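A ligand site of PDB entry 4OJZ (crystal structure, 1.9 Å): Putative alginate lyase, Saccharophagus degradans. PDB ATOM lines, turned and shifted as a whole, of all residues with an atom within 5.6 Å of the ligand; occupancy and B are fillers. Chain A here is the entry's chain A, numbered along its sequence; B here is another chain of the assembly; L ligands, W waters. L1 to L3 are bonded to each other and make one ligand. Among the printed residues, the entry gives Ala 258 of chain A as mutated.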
ATOM      1  N   HIS A  86     -12.805  18.816  18.874  1.00  0.00           N
ATOM      2  CA  HIS A  86     -12.087  17.689  18.277  1.00  0.00           C
ATOM      3  C   HIS A  86     -12.193  16.435  19.153  1.00  0.00           C
ATOM      4  O   HIS A  86     -12.647  15.385  18.698  1.00  0.00           O
ATOM      5  CB  HIS A  86     -10.611  18.059  18.076  1.00  0.00           C
ATOM      6  CG  HIS A  86      -9.828  17.060  17.285  1.00  0.00           C
ATOM      7  ND1 HIS A  86      -9.785  17.072  15.905  1.00  0.00           N
ATOM      8  CD2 HIS A  86      -9.041  16.036  17.687  1.00  0.00           C
ATOM      9  CE1 HIS A  86      -9.015  16.086  15.489  1.00  0.00           C
ATOM     10  NE2 HIS A  86      -8.550  15.440  16.545  1.00  0.00           N
ATOM     11  N   LYS A  90     -14.652  12.960  19.128  1.00  0.00           N
ATOM     12  CA  LYS A  90     -13.952  11.685  19.289  1.00  0.00           C
ATOM     13  C   LYS A  90     -14.578  10.845  20.401  1.00  0.00           C
ATOM     14  O   LYS A  90     -14.887   9.663  20.192  1.00  0.00           O
ATOM     15  CB  LYS A  90     -12.453  11.898  19.528  1.00  0.00           C
ATOM     16  CG  LYS A  90     -11.651  12.139  18.251  1.00  0.00           C
ATOM     17  CD  LYS A  90     -10.268  12.719  18.522  1.00  0.00           C
ATOM     18  CE  LYS A  90      -9.371  11.721  19.255  1.00  0.00           C
ATOM     19  NZ  LYS A  90      -7.952  12.189  19.364  1.00  0.00           N
ATOM     20  N   LYS A 136      -7.874  22.020   7.990  1.00  0.00           N
ATOM     21  CA  LYS A 136      -6.592  21.715   7.373  1.00  0.00           C
ATOM     22  C   LYS A 136      -6.686  22.083   5.896  1.00  0.00           C
ATOM     23  O   LYS A 136      -7.653  21.741   5.224  1.00  0.00           O
ATOM     24  CB  LYS A 136      -6.279  20.233   7.538  1.00  0.00           C
ATOM     25  CG  LYS A 136      -4.882  19.826   7.110  1.00  0.00           C
ATOM     26  CD  LYS A 136      -4.548  18.442   7.653  1.00  0.00           C
ATOM     27  CE  LYS A 136      -3.758  17.619   6.645  1.00  0.00           C
ATOM     28  NZ  LYS A 136      -2.427  18.198   6.356  1.00  0.00           N
ATOM     29  N   GLN A 138      -4.973  21.091   3.199  1.00  0.00           N
ATOM     30  CA  GLN A 138      -4.861  20.017   2.205  1.00  0.00           C
ATOM     31  C   GLN A 138      -6.115  19.149   2.083  1.00  0.00           C
ATOM     32  O   GLN A 138      -6.496  18.756   0.968  1.00  0.00           O
ATOM     33  CB  GLN A 138      -3.639  19.135   2.481  1.00  0.00           C
ATOM     34  CG  GLN A 138      -2.294  19.818   2.240  1.00  0.00           C
ATOM     35  CD  GLN A 138      -1.783  20.598   3.449  1.00  0.00           C
ATOM     36  OE1 GLN A 138      -2.412  20.600   4.522  1.00  0.00           O
ATOM     37  NE2 GLN A 138      -0.638  21.257   3.292  1.00  0.00           N
ATOM     38  N   TRP A 145     -11.318  19.255  11.898  1.00  0.00           N
ATOM     39  CA  TRP A 145     -10.467  20.161  11.127  1.00  0.00           C
ATOM     40  C   TRP A 145      -9.941  19.529   9.823  1.00  0.00           C
ATOM     41  O   TRP A 145      -9.708  20.210   8.827  1.00  0.00           O
ATOM     42  CB  TRP A 145      -9.316  20.671  11.998  1.00  0.00           C
ATOM     43  CG  TRP A 145      -8.221  19.670  12.230  1.00  0.00           C
ATOM     44  CD1 TRP A 145      -8.319  18.488  12.908  1.00  0.00           C
ATOM     45  CD2 TRP A 145      -6.869  19.768  11.787  1.00  0.00           C
ATOM     46  NE1 TRP A 145      -7.103  17.839  12.915  1.00  0.00           N
ATOM     47  CE2 TRP A 145      -6.196  18.596  12.230  1.00  0.00           C
ATOM     48  CE3 TRP A 145      -6.153  20.729  11.059  1.00  0.00           C
ATOM     49  CZ2 TRP A 145      -4.849  18.370  11.963  1.00  0.00           C
ATOM     50  CZ3 TRP A 145      -4.809  20.493  10.794  1.00  0.00           C
ATOM     51  CH2 TRP A 145      -4.171  19.325  11.251  1.00  0.00           C
ATOM     52  N   GLN A 146      -9.779  18.213   9.838  1.00  0.00           N
ATOM     53  CA  GLN A 146      -9.331  17.464   8.668  1.00  0.00           C
ATOM     54  C   GLN A 146     -10.283  16.292   8.437  1.00  0.00           C
ATOM     55  O   GLN A 146     -10.883  15.781   9.376  1.00  0.00           O
ATOM     56  CB  GLN A 146      -7.883  16.983   8.852  1.00  0.00           C
ATOM     57  CG  GLN A 146      -7.681  16.016  10.013  1.00  0.00           C
ATOM     58  CD  GLN A 146      -6.260  15.486  10.132  1.00  0.00           C
ATOM     59  OE1 GLN A 146      -5.458  15.601   9.207  1.00  0.00           O
ATOM     60  NE2 GLN A 146      -5.955  14.904  11.288  1.00  0.00           N
ATOM     61  N   LEU A 148      -9.646  13.288   7.692  1.00  0.00           N
ATOM     62  CA  LEU A 148      -9.175  12.019   8.272  1.00  0.00           C
ATOM     63  C   LEU A 148      -9.996  11.612   9.498  1.00  0.00           C
ATOM     64  O   LEU A 148     -10.510  10.492   9.559  1.00  0.00           O
ATOM     65  CB  LEU A 148      -7.678  12.096   8.624  1.00  0.00           C
ATOM     66  CG  LEU A 148      -7.062  10.879   9.312  1.00  0.00           C
ATOM     67  CD1 LEU A 148      -7.086   9.653   8.398  1.00  0.00           C
ATOM     68  CD2 LEU A 148      -5.634  11.193   9.753  1.00  0.00           C
ATOM     69  N   ASN A 149     -10.111  12.532  10.472  1.00  0.00           N
ATOM     70  CA  ASN A 149     -10.847  12.248  11.701  1.00  0.00           C
ATOM     71  C   ASN A 149     -12.347  12.053  11.446  1.00  0.00           C
ATOM     72  O   ASN A 149     -13.004  11.281  12.141  1.00  0.00           O
ATOM     73  CB  ASN A 149     -10.617  13.343  12.756  1.00  0.00           C
ATOM     74  CG  ASN A 149      -9.148  13.531  13.081  1.00  0.00           C
ATOM     75  OD1 ASN A 149      -8.519  14.483  12.625  1.00  0.00           O
ATOM     76  ND2 ASN A 149      -8.583  12.605  13.846  1.00  0.00           N
ATOM     77  N   LYS A 198      -7.252   8.467  -3.448  1.00  0.00           N
ATOM     78  CA  LYS A 198      -5.832   8.465  -3.088  1.00  0.00           C
ATOM     79  C   LYS A 198      -5.376   7.048  -2.755  1.00  0.00           C
ATOM     80  O   LYS A 198      -6.070   6.299  -2.062  1.00  0.00           O
ATOM     81  CB  LYS A 198      -5.563   9.393  -1.905  1.00  0.00           C
ATOM     82  CG  LYS A 198      -4.217  10.105  -1.964  1.00  0.00           C
ATOM     83  CD  LYS A 198      -4.009  10.995  -0.749  1.00  0.00           C
ATOM     84  CE  LYS A 198      -2.591  11.543  -0.716  1.00  0.00           C
ATOM     85  NZ  LYS A 198      -2.233  12.020   0.645  1.00  0.00           N
ATOM     86  N   HIS A 200      -3.233   5.707  -0.552  1.00  0.00           N
ATOM     87  CA  HIS A 200      -2.614   6.219   0.670  1.00  0.00           C
ATOM     88  C   HIS A 200      -3.542   5.819   1.821  1.00  0.00           C
ATOM     89  O   HIS A 200      -4.730   5.571   1.587  1.00  0.00           O
ATOM     90  CB  HIS A 200      -2.501   7.746   0.553  1.00  0.00           C
ATOM     91  CG  HIS A 200      -1.780   8.400   1.690  1.00  0.00           C
ATOM     92  ND1 HIS A 200      -2.422   8.859   2.821  1.00  0.00           N
ATOM     93  CD2 HIS A 200      -0.465   8.718   1.843  1.00  0.00           C
ATOM     94  CE1 HIS A 200      -1.538   9.401   3.641  1.00  0.00           C
ATOM     95  NE2 HIS A 200      -0.345   9.328   3.068  1.00  0.00           N
ATOM     96  N   ASN A 201      -3.036   5.746   3.050  1.00  0.00           N
ATOM     97  CA  ASN A 201      -3.925   5.323   4.152  1.00  0.00           C
ATOM     98  C   ASN A 201      -5.071   6.292   4.478  1.00  0.00           C
ATOM     99  O   ASN A 201      -6.074   5.876   5.059  1.00  0.00           O
ATOM    100  CB  ASN A 201      -3.190   4.820   5.420  1.00  0.00           C
ATOM    101  CG  ASN A 201      -2.324   5.871   6.092  1.00  0.00           C
ATOM    102  OD1 ASN A 201      -2.472   7.072   5.869  1.00  0.00           O
ATOM    103  ND2 ASN A 201      -1.403   5.408   6.942  1.00  0.00           N
ATOM    104  N   HIS A 202      -4.948   7.558   4.068  1.00  0.00           N
ATOM    105  CA  HIS A 202      -6.067   8.495   4.144  1.00  0.00           C
ATOM    106  C   HIS A 202      -7.178   8.081   3.180  1.00  0.00           C
ATOM    107  O   HIS A 202      -8.364   8.291   3.463  1.00  0.00           O
ATOM    108  CB  HIS A 202      -5.607   9.931   3.877  1.00  0.00           C
ATOM    109  CG  HIS A 202      -4.767  10.505   4.976  1.00  0.00           C
ATOM    110  ND1 HIS A 202      -4.679  11.851   5.212  1.00  0.00           N
ATOM    111  CD2 HIS A 202      -3.991   9.904   5.911  1.00  0.00           C
ATOM    112  CE1 HIS A 202      -3.884  12.070   6.245  1.00  0.00           C
ATOM    113  NE2 HIS A 202      -3.445  10.898   6.685  1.00  0.00           N
ATOM    114  N   TYR A 257       4.638   2.822  12.306  1.00  0.00           N
ATOM    115  CA  TYR A 257       3.688   3.787  12.851  1.00  0.00           C
ATOM    116  C   TYR A 257       2.503   4.003  11.905  1.00  0.00           C
ATOM    117  O   TYR A 257       1.356   4.045  12.359  1.00  0.00           O
ATOM    118  CB  TYR A 257       4.388   5.116  13.179  1.00  0.00           C
ATOM    119  CG  TYR A 257       3.500   6.137  13.869  1.00  0.00           C
ATOM    120  CD1 TYR A 257       3.267   6.089  15.245  1.00  0.00           C
ATOM    121  CD2 TYR A 257       2.900   7.166  13.132  1.00  0.00           C
ATOM    122  CE1 TYR A 257       2.460   7.026  15.869  1.00  0.00           C
ATOM    123  CE2 TYR A 257       2.096   8.112  13.754  1.00  0.00           C
ATOM    124  CZ  TYR A 257       1.880   8.035  15.120  1.00  0.00           C
ATOM    125  OH  TYR A 257       1.067   8.969  15.722  1.00  0.00           O
ATOM    126  N   ALA A 258       2.795   4.129  10.625  1.00  0.00           N
ATOM    127  CA  ALA A 258       1.759   4.211   9.587  1.00  0.00           C
ATOM    128  C   ALA A 258       1.080   2.866   9.363  1.00  0.00           C
ATOM    129  O   ALA A 258      -0.129   2.801   9.147  1.00  0.00           O
ATOM    130  CB  ALA A 258       2.338   4.725   8.294  1.00  0.00           C
ATOM    131  N   ARG A 260       0.392   0.335  11.474  1.00  0.00           N
ATOM    132  CA  ARG A 260      -0.631   0.029  12.474  1.00  0.00           C
ATOM    133  C   ARG A 260      -1.880   0.894  12.324  1.00  0.00           C
ATOM    134  O   ARG A 260      -2.982   0.456  12.617  1.00  0.00           O
ATOM    135  CB  ARG A 260      -0.075   0.085  13.919  1.00  0.00           C
ATOM    136  CG  ARG A 260       0.407   1.447  14.417  1.00  0.00           C
ATOM    137  CD  ARG A 260      -0.715   2.380  14.855  1.00  0.00           C
ATOM    138  NE  ARG A 260      -0.331   3.776  14.637  1.00  0.00           N
ATOM    139  CZ  ARG A 260      -1.035   4.849  15.009  1.00  0.00           C
ATOM    140  NH1 ARG A 260      -2.206   4.720  15.624  1.00  0.00           N
ATOM    141  NH2 ARG A 260      -0.555   6.058  14.768  1.00  0.00           N
ATOM    142  N   TYR A 261      -1.686   2.137  11.870  1.00  0.00           N
ATOM    143  CA  TYR A 261      -2.801   3.054  11.668  1.00  0.00           C
ATOM    144  C   TYR A 261      -3.642   2.621  10.476  1.00  0.00           C
ATOM    145  O   TYR A 261      -4.879   2.556  10.562  1.00  0.00           O
ATOM    146  CB  TYR A 261      -2.291   4.497  11.504  1.00  0.00           C
ATOM    147  CG  TYR A 261      -3.381   5.558  11.551  1.00  0.00           C
ATOM    148  CD1 TYR A 261      -4.315   5.586  12.589  1.00  0.00           C
ATOM    149  CD2 TYR A 261      -3.456   6.559  10.585  1.00  0.00           C
ATOM    150  CE1 TYR A 261      -5.315   6.556  12.648  1.00  0.00           C
ATOM    151  CE2 TYR A 261      -4.451   7.536  10.632  1.00  0.00           C
ATOM    152  CZ  TYR A 261      -5.361   7.535  11.673  1.00  0.00           C
ATOM    153  OH  TYR A 261      -6.351   8.503  11.734  1.00  0.00           O
ATOM    154  N   ASP A 311       8.531   8.807  10.486  1.00  0.00           N
ATOM    155  CA  ASP A 311       7.533   9.476  11.318  1.00  0.00           C
ATOM    156  C   ASP A 311       6.960   8.447  12.283  1.00  0.00           C
ATOM    157  O   ASP A 311       6.333   7.473  11.869  1.00  0.00           O
ATOM    158  CB  ASP A 311       6.422  10.036  10.436  1.00  0.00           C
ATOM    159  CG  ASP A 311       5.312  10.660  11.239  1.00  0.00           C
ATOM    160  OD1 ASP A 311       5.592  11.691  11.887  1.00  0.00           O
ATOM    161  OD2 ASP A 311       4.176  10.130  11.212  1.00  0.00           O
ATOM    162  N   LEU A 313       5.789   8.005  16.805  1.00  0.00           N
ATOM    163  CA  LEU A 313       5.795   8.462  18.188  1.00  0.00           C
ATOM    164  C   LEU A 313       6.165   7.323  19.113  1.00  0.00           C
ATOM    165  O   LEU A 313       5.626   6.214  18.997  1.00  0.00           O
ATOM    166  CB  LEU A 313       4.451   9.112  18.578  1.00  0.00           C
ATOM    167  CG  LEU A 313       4.051  10.354  17.787  1.00  0.00           C
ATOM    168  CD1 LEU A 313       2.658  10.829  18.187  1.00  0.00           C
ATOM    169  CD2 LEU A 313       5.055  11.495  17.953  1.00  0.00           C
ATOM    170  N   HIS A 413       6.800  11.270   4.943  1.00  0.00           N
ATOM    171  CA  HIS A 413       6.988  10.784   6.313  1.00  0.00           C
ATOM    172  C   HIS A 413       8.386  10.187   6.532  1.00  0.00           C
ATOM    173  O   HIS A 413       8.737   9.844   7.671  1.00  0.00           O
ATOM    174  CB  HIS A 413       5.915   9.748   6.666  1.00  0.00           C
ATOM    175  CG  HIS A 413       4.525  10.299   6.736  1.00  0.00           C
ATOM    176  ND1 HIS A 413       4.198  11.394   7.514  1.00  0.00           N
ATOM    177  CD2 HIS A 413       3.378   9.912   6.128  1.00  0.00           C
ATOM    178  CE1 HIS A 413       2.905  11.651   7.371  1.00  0.00           C
ATOM    179  NE2 HIS A 413       2.394  10.772   6.539  1.00  0.00           N
ATOM    180  N   ARG A 438       6.679  15.960  17.639  1.00  0.00           N
ATOM    181  CA  ARG A 438       5.225  16.104  17.624  1.00  0.00           C
ATOM    182  C   ARG A 438       4.672  15.601  18.951  1.00  0.00           C
ATOM    183  O   ARG A 438       5.183  14.639  19.525  1.00  0.00           O
ATOM    184  CB  ARG A 438       4.630  15.296  16.459  1.00  0.00           C
ATOM    185  CG  ARG A 438       3.113  15.284  16.370  1.00  0.00           C
ATOM    186  CD  ARG A 438       2.670  14.389  15.228  1.00  0.00           C
ATOM    187  NE  ARG A 438       1.213  14.403  15.059  1.00  0.00           N
ATOM    188  CZ  ARG A 438       0.531  13.487  14.395  1.00  0.00           C
ATOM    189  NH1 ARG A 438       1.157  12.450  13.828  1.00  0.00           N
ATOM    190  NH2 ARG A 438      -0.794  13.594  14.299  1.00  0.00           N
ATOM    191  N   LEU A 440       1.152  14.293  20.271  1.00  0.00           N
ATOM    192  CA  LEU A 440      -0.150  13.829  19.771  1.00  0.00           C
ATOM    193  C   LEU A 440      -1.320  14.465  20.495  1.00  0.00           C
ATOM    194  O   LEU A 440      -1.436  14.334  21.716  1.00  0.00           O
ATOM    195  CB  LEU A 440      -0.258  12.309  19.877  1.00  0.00           C
ATOM    196  CG  LEU A 440      -1.462  11.681  19.167  1.00  0.00           C
ATOM    197  CD1 LEU A 440      -1.275  11.660  17.655  1.00  0.00           C
ATOM    198  CD2 LEU A 440      -1.663  10.272  19.688  1.00  0.00           C
ATOM    199  N   ASN A 441      -2.175  15.154  19.742  1.00  0.00           N
ATOM    200  CA  ASN A 441      -3.377  15.771  20.286  1.00  0.00           C
ATOM    201  C   ASN A 441      -3.129  16.753  21.439  1.00  0.00           C
ATOM    202  O   ASN A 441      -3.983  16.941  22.299  1.00  0.00           O
ATOM    203  CB  ASN A 441      -4.388  14.692  20.726  1.00  0.00           C
ATOM    204  CG  ASN A 441      -4.760  13.756  19.598  1.00  0.00           C
ATOM    205  OD1 ASN A 441      -4.887  12.540  19.793  1.00  0.00           O
ATOM    206  ND2 ASN A 441      -4.943  14.311  18.400  1.00  0.00           N
ATOM    207  N   HIS A 449       0.166  18.857  15.692  1.00  0.00           N
ATOM    208  CA  HIS A 449       0.726  18.618  14.366  1.00  0.00           C
ATOM    209  C   HIS A 449       2.257  18.577  14.431  1.00  0.00           C
ATOM    210  O   HIS A 449       2.839  18.758  15.507  1.00  0.00           O
ATOM    211  CB  HIS A 449       0.211  19.670  13.375  1.00  0.00           C
ATOM    212  CG  HIS A 449       0.268  19.236  11.944  1.00  0.00           C
ATOM    213  ND1 HIS A 449      -0.419  18.157  11.452  1.00  0.00           N
ATOM    214  CD2 HIS A 449       0.945  19.760  10.889  1.00  0.00           C
ATOM    215  CE1 HIS A 449      -0.184  18.019  10.162  1.00  0.00           C
ATOM    216  NE2 HIS A 449       0.648  18.979   9.796  1.00  0.00           N
ATOM    217  N   TYR A 450       2.910  18.318  13.298  1.00  0.00           N
ATOM    218  CA  TYR A 450       4.365  18.264  13.236  1.00  0.00           C
ATOM    219  C   TYR A 450       4.966  19.629  13.534  1.00  0.00           C
ATOM    220  O   TYR A 450       4.556  20.628  12.937  1.00  0.00           O
ATOM    221  CB  TYR A 450       4.864  17.758  11.879  1.00  0.00           C
ATOM    222  CG  TYR A 450       4.201  16.470  11.452  1.00  0.00           C
ATOM    223  CD1 TYR A 450       4.572  15.251  12.019  1.00  0.00           C
ATOM    224  CD2 TYR A 450       3.205  16.478  10.474  1.00  0.00           C
ATOM    225  CE1 TYR A 450       3.961  14.072  11.623  1.00  0.00           C
ATOM    226  CE2 TYR A 450       2.594  15.298  10.079  1.00  0.00           C
ATOM    227  CZ  TYR A 450       2.981  14.108  10.651  1.00  0.00           C
ATOM    228  OH  TYR A 450       2.373  12.937  10.254  1.00  0.00           O
ATOM    229  N   GLU B 667      -4.996   7.429  22.107  1.00  0.00           N
ATOM    230  CA  GLU B 667      -4.873   8.675  21.321  1.00  0.00           C
ATOM    231  C   GLU B 667      -6.002   9.658  21.636  1.00  0.00           C
ATOM    232  O   GLU B 667      -6.755  10.082  20.757  1.00  0.00           O
ATOM    233  CB  GLU B 667      -4.747   8.384  19.810  1.00  0.00           C
ATOM    234  CG  GLU B 667      -3.655   7.350  19.501  1.00  0.00           C
ATOM    235  CD  GLU B 667      -3.152   7.396  18.073  1.00  0.00           C
ATOM    236  OE1 GLU B 667      -3.691   8.147  17.236  1.00  0.00           O
ATOM    237  OE2 GLU B 667      -2.176   6.660  17.773  1.00  0.00           O
HETATM  238  C1  LIG L   1      -1.086  15.393   3.661  1.00  0.00           C
HETATM  239  C2  LIG L   1      -1.416  13.958   4.122  1.00  0.00           C
HETATM  240  O1  LIG L   1      -1.603  13.113   2.994  1.00  0.00           O
HETATM  241  C3  LIG L   1      -0.349  13.358   5.049  1.00  0.00           C
HETATM  242  O2  LIG L   1       0.817  12.964   4.298  1.00  0.00           O
HETATM  243  C4  LIG L   1       0.055  14.340   6.138  1.00  0.00           C
HETATM  244  O3  LIG L   1      -1.071  14.595   7.000  1.00  0.00           O
HETATM  245  C5  LIG L   1       0.482  15.657   5.485  1.00  0.00           C
HETATM  246  O4  LIG L   1      -0.636  16.190   4.758  1.00  0.00           O
HETATM  247  C6  LIG L   1       0.902  16.656   6.530  1.00  0.00           C
HETATM  248  O5  LIG L   1       0.128  17.600   6.799  1.00  0.00           O
HETATM  249  O6  LIG L   1       2.008  16.507   7.082  1.00  0.00           O
HETATM  250  O7  LIG L   1      -0.080  15.396   2.627  1.00  0.00           O
HETATM  251  C1  LG2 L   2      -0.904  13.919   8.262  1.00  0.00           C
HETATM  252  C2  LG2 L   2      -1.931  14.440   9.258  1.00  0.00           C
HETATM  253  O1  LG2 L   2      -3.237  14.219   8.730  1.00  0.00           O
HETATM  254  C3  LG2 L   2      -1.810  13.711  10.599  1.00  0.00           C
HETATM  255  O2  LG2 L   2      -2.930  14.031  11.423  1.00  0.00           O
HETATM  256  C4  LG2 L   2      -1.693  12.182  10.413  1.00  0.00           C
HETATM  257  O3  LG2 L   2      -1.223  11.576  11.607  1.00  0.00           O
HETATM  258  C5  LG2 L   2      -0.693  11.818   9.314  1.00  0.00           C
HETATM  259  O4  LG2 L   2      -1.036  12.502   8.122  1.00  0.00           O
HETATM  260  C6  LG2 L   2      -0.720  10.335   9.075  1.00  0.00           C
HETATM  261  O5  LG2 L   2      -1.664   9.846   8.408  1.00  0.00           O
HETATM  262  O6  LG2 L   2       0.196   9.640   9.556  1.00  0.00           O
HETATM  263  C1  LG3 L   3      -2.255  10.800  12.221  1.00  0.00           C
HETATM  264  C2  LG3 L   3      -1.632   9.747  13.128  1.00  0.00           C
HETATM  265  O1  LG3 L   3      -0.802  10.406  14.105  1.00  0.00           O
HETATM  266  C3  LG3 L   3      -2.719   8.947  13.844  1.00  0.00           C
HETATM  267  O2  LG3 L   3      -2.135   8.287  14.959  1.00  0.00           O
HETATM  268  C4  LG3 L   3      -3.879   9.797  14.382  1.00  0.00           C
HETATM  269  C5  LG3 L   3      -4.265  10.950  13.450  1.00  0.00           C
HETATM  270  O3  LG3 L   3      -3.100  11.634  13.004  1.00  0.00           O
HETATM  271  C6  LG3 L   3      -5.159  11.953  14.102  1.00  0.00           C
HETATM  272  O4  LG3 L   3      -4.993  13.164  13.799  1.00  0.00           O
HETATM  273  O5  LG3 L   3      -6.044  11.557  14.900  1.00  0.00           O
HETATM  274  O   HOH W   1      -6.848  13.324  16.843  1.00  0.00           O
HETATM  275  O   HOH W   2      -5.237  10.715  17.358  1.00  0.00           O
HETATM  276  O   HOH W   3      -5.869  15.739  14.493  1.00  0.00           O
HETATM  277  O   HOH W   4      -7.247   9.100  14.225  1.00  0.00           O
HETATM  278  O   HOH W   5      -1.817  16.400  12.825  1.00  0.00           O
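NZ of Lys 198 lies within hydrogen-bond range of O1 of LIG L1 (2.7 Å). NH2 of Arg 260 is in hydrogen-bond range of O2 of LG3 L3 (2.7 Å). The guanidinium group (NH1) of Arg 438 is in hydrogen-bond range of an oxygen (O1) of LG3 L3 (2.8 Å). O5 of LIG L1 lies within salt-bridge range of NZ of Lys 136 (2.7 Å). NE2 of His 202 lies within hydrogen-bond range of O5 of LG2 L2 (2.7 Å). The side-chain carboxylate of Glu 667 of chain B is in hydrogen-bond range of an oxygen (O2) of LG3 L3. OE1 of Gln 146 sits at hydrogen-bond distance from O1 of LG2 L2 (2.7 Å). An oxygen (O5) of LIG L1 is in hydrogen-bond range of a ring nitrogen (NE2) of His 449 (3.3 Å). ND2 of Asn 149 lies within hydrogen-bond range of O5 of LG3 L3, at 2.9 Å. The side-chain hydroxyl of Tyr 257 sits at hydrogen-bond distance from an oxygen (O1) of LG3 L3, 2.9 Å away.
The guanidinium group of Arg 260 lies within salt-bridge range of the side-chain carboxylate of Glu 667 of chain B (2.9 Å). The backbone carbonyl oxygen (O) of Trp 145 is in hydrogen-bond range of the backbone NH (N) of Lys 136, at 2.7 Å. NZ of Lys 136 lies within hydrogen-bond range of OE1 of Gln 138 (3.0 Å). The side-chain amide nitrogen of Gln 146 is in hydrogen-bond range of the side-chain amide oxygen of Asn 149 (2.9 Å). O of Glu 667 of chain B sits close to OD1 of Asn 441, at 3.2 Å. The backbone NH (N) of Asp 311 sits at hydrogen-bond distance from the backbone carbonyl oxygen (O) of His 413 (3.0 Å). O of Tyr 257 sits at hydrogen-bond distance from NE of Arg 260 (2.8 Å). The backbone NH of His 202 is in hydrogen-bond range of a ring nitrogen (ND1) of His 200.
CD2 of Leu 148 touches C5 of LG3 L3, 3.9 Å away. CE1 of His 200 touches O1 of LIG L1, at 3.8 Å. OD1 of Asn 201 touches O5 of LG2 L2, 3.8 Å away. OH of Tyr 261 touches C5 of LG3 L3 (3.6 Å). NE2 of His 413 touches O2 of LIG L1, 3.5 Å away. CD1 of Leu 440 touches O1 of LG3 L3 (3.8 Å). CE2 of Tyr 450 touches O6 of LIG L1, 3.3 Å away. Hydrophobic or aromatic side chains within 4 Å of the ligand: Leu 148, His 200, His 202, Tyr 257, Tyr 261, His 413, Leu 440, His 449 and Tyr 450. Within 4 Å of the ligand: Lys 136, Gln 146, Leu 148, Asn 149, Lys 198, His 200, Asn 201, His 202, Tyr 257, Arg 260, Tyr 261, His 413, Arg 438, Leu 440, His 449, Tyr 450 and Glu 667 of chain B. Along chain A the residues within 4 Å of the ligand span positions 136 to 450.
Water W2 lies within hydrogen-bond range of an oxygen (O5) of LG3 L3 (2.7 Å), the side-chain carboxylate (OE1) of Glu 667 of chain B (3.0 Å) and the side-chain amide oxygen (OD1) of Asn 441 (3.1 Å). Water W1 lies within hydrogen-bond range of the side-chain amide nitrogen of Asn 441 (2.7 Å), a ring nitrogen (NE2) of His 86 (2.7 Å), an oxygen (O5) of LG3 L3 (2.7 Å) and the side-chain amino group of Lys 90 (3.0 Å). Water W3 lies within hydrogen-bond range of an oxygen (O4) of LG3 L3, the indole nitrogen (NE1) of Trp 145, the side-chain amide nitrogen (NE2) of Gln 146, a ring nitrogen (NE2) of His 86 and the side-chain amide oxygen (OD1) of Asn 149. Water W4 lies within hydrogen-bond range of OH of Tyr 261 and O5 of LG3 L3. Water W5 lies within hydrogen-bond range of ND1 of His 449, O2 of LG2 L2 and NH2 of Arg 438.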
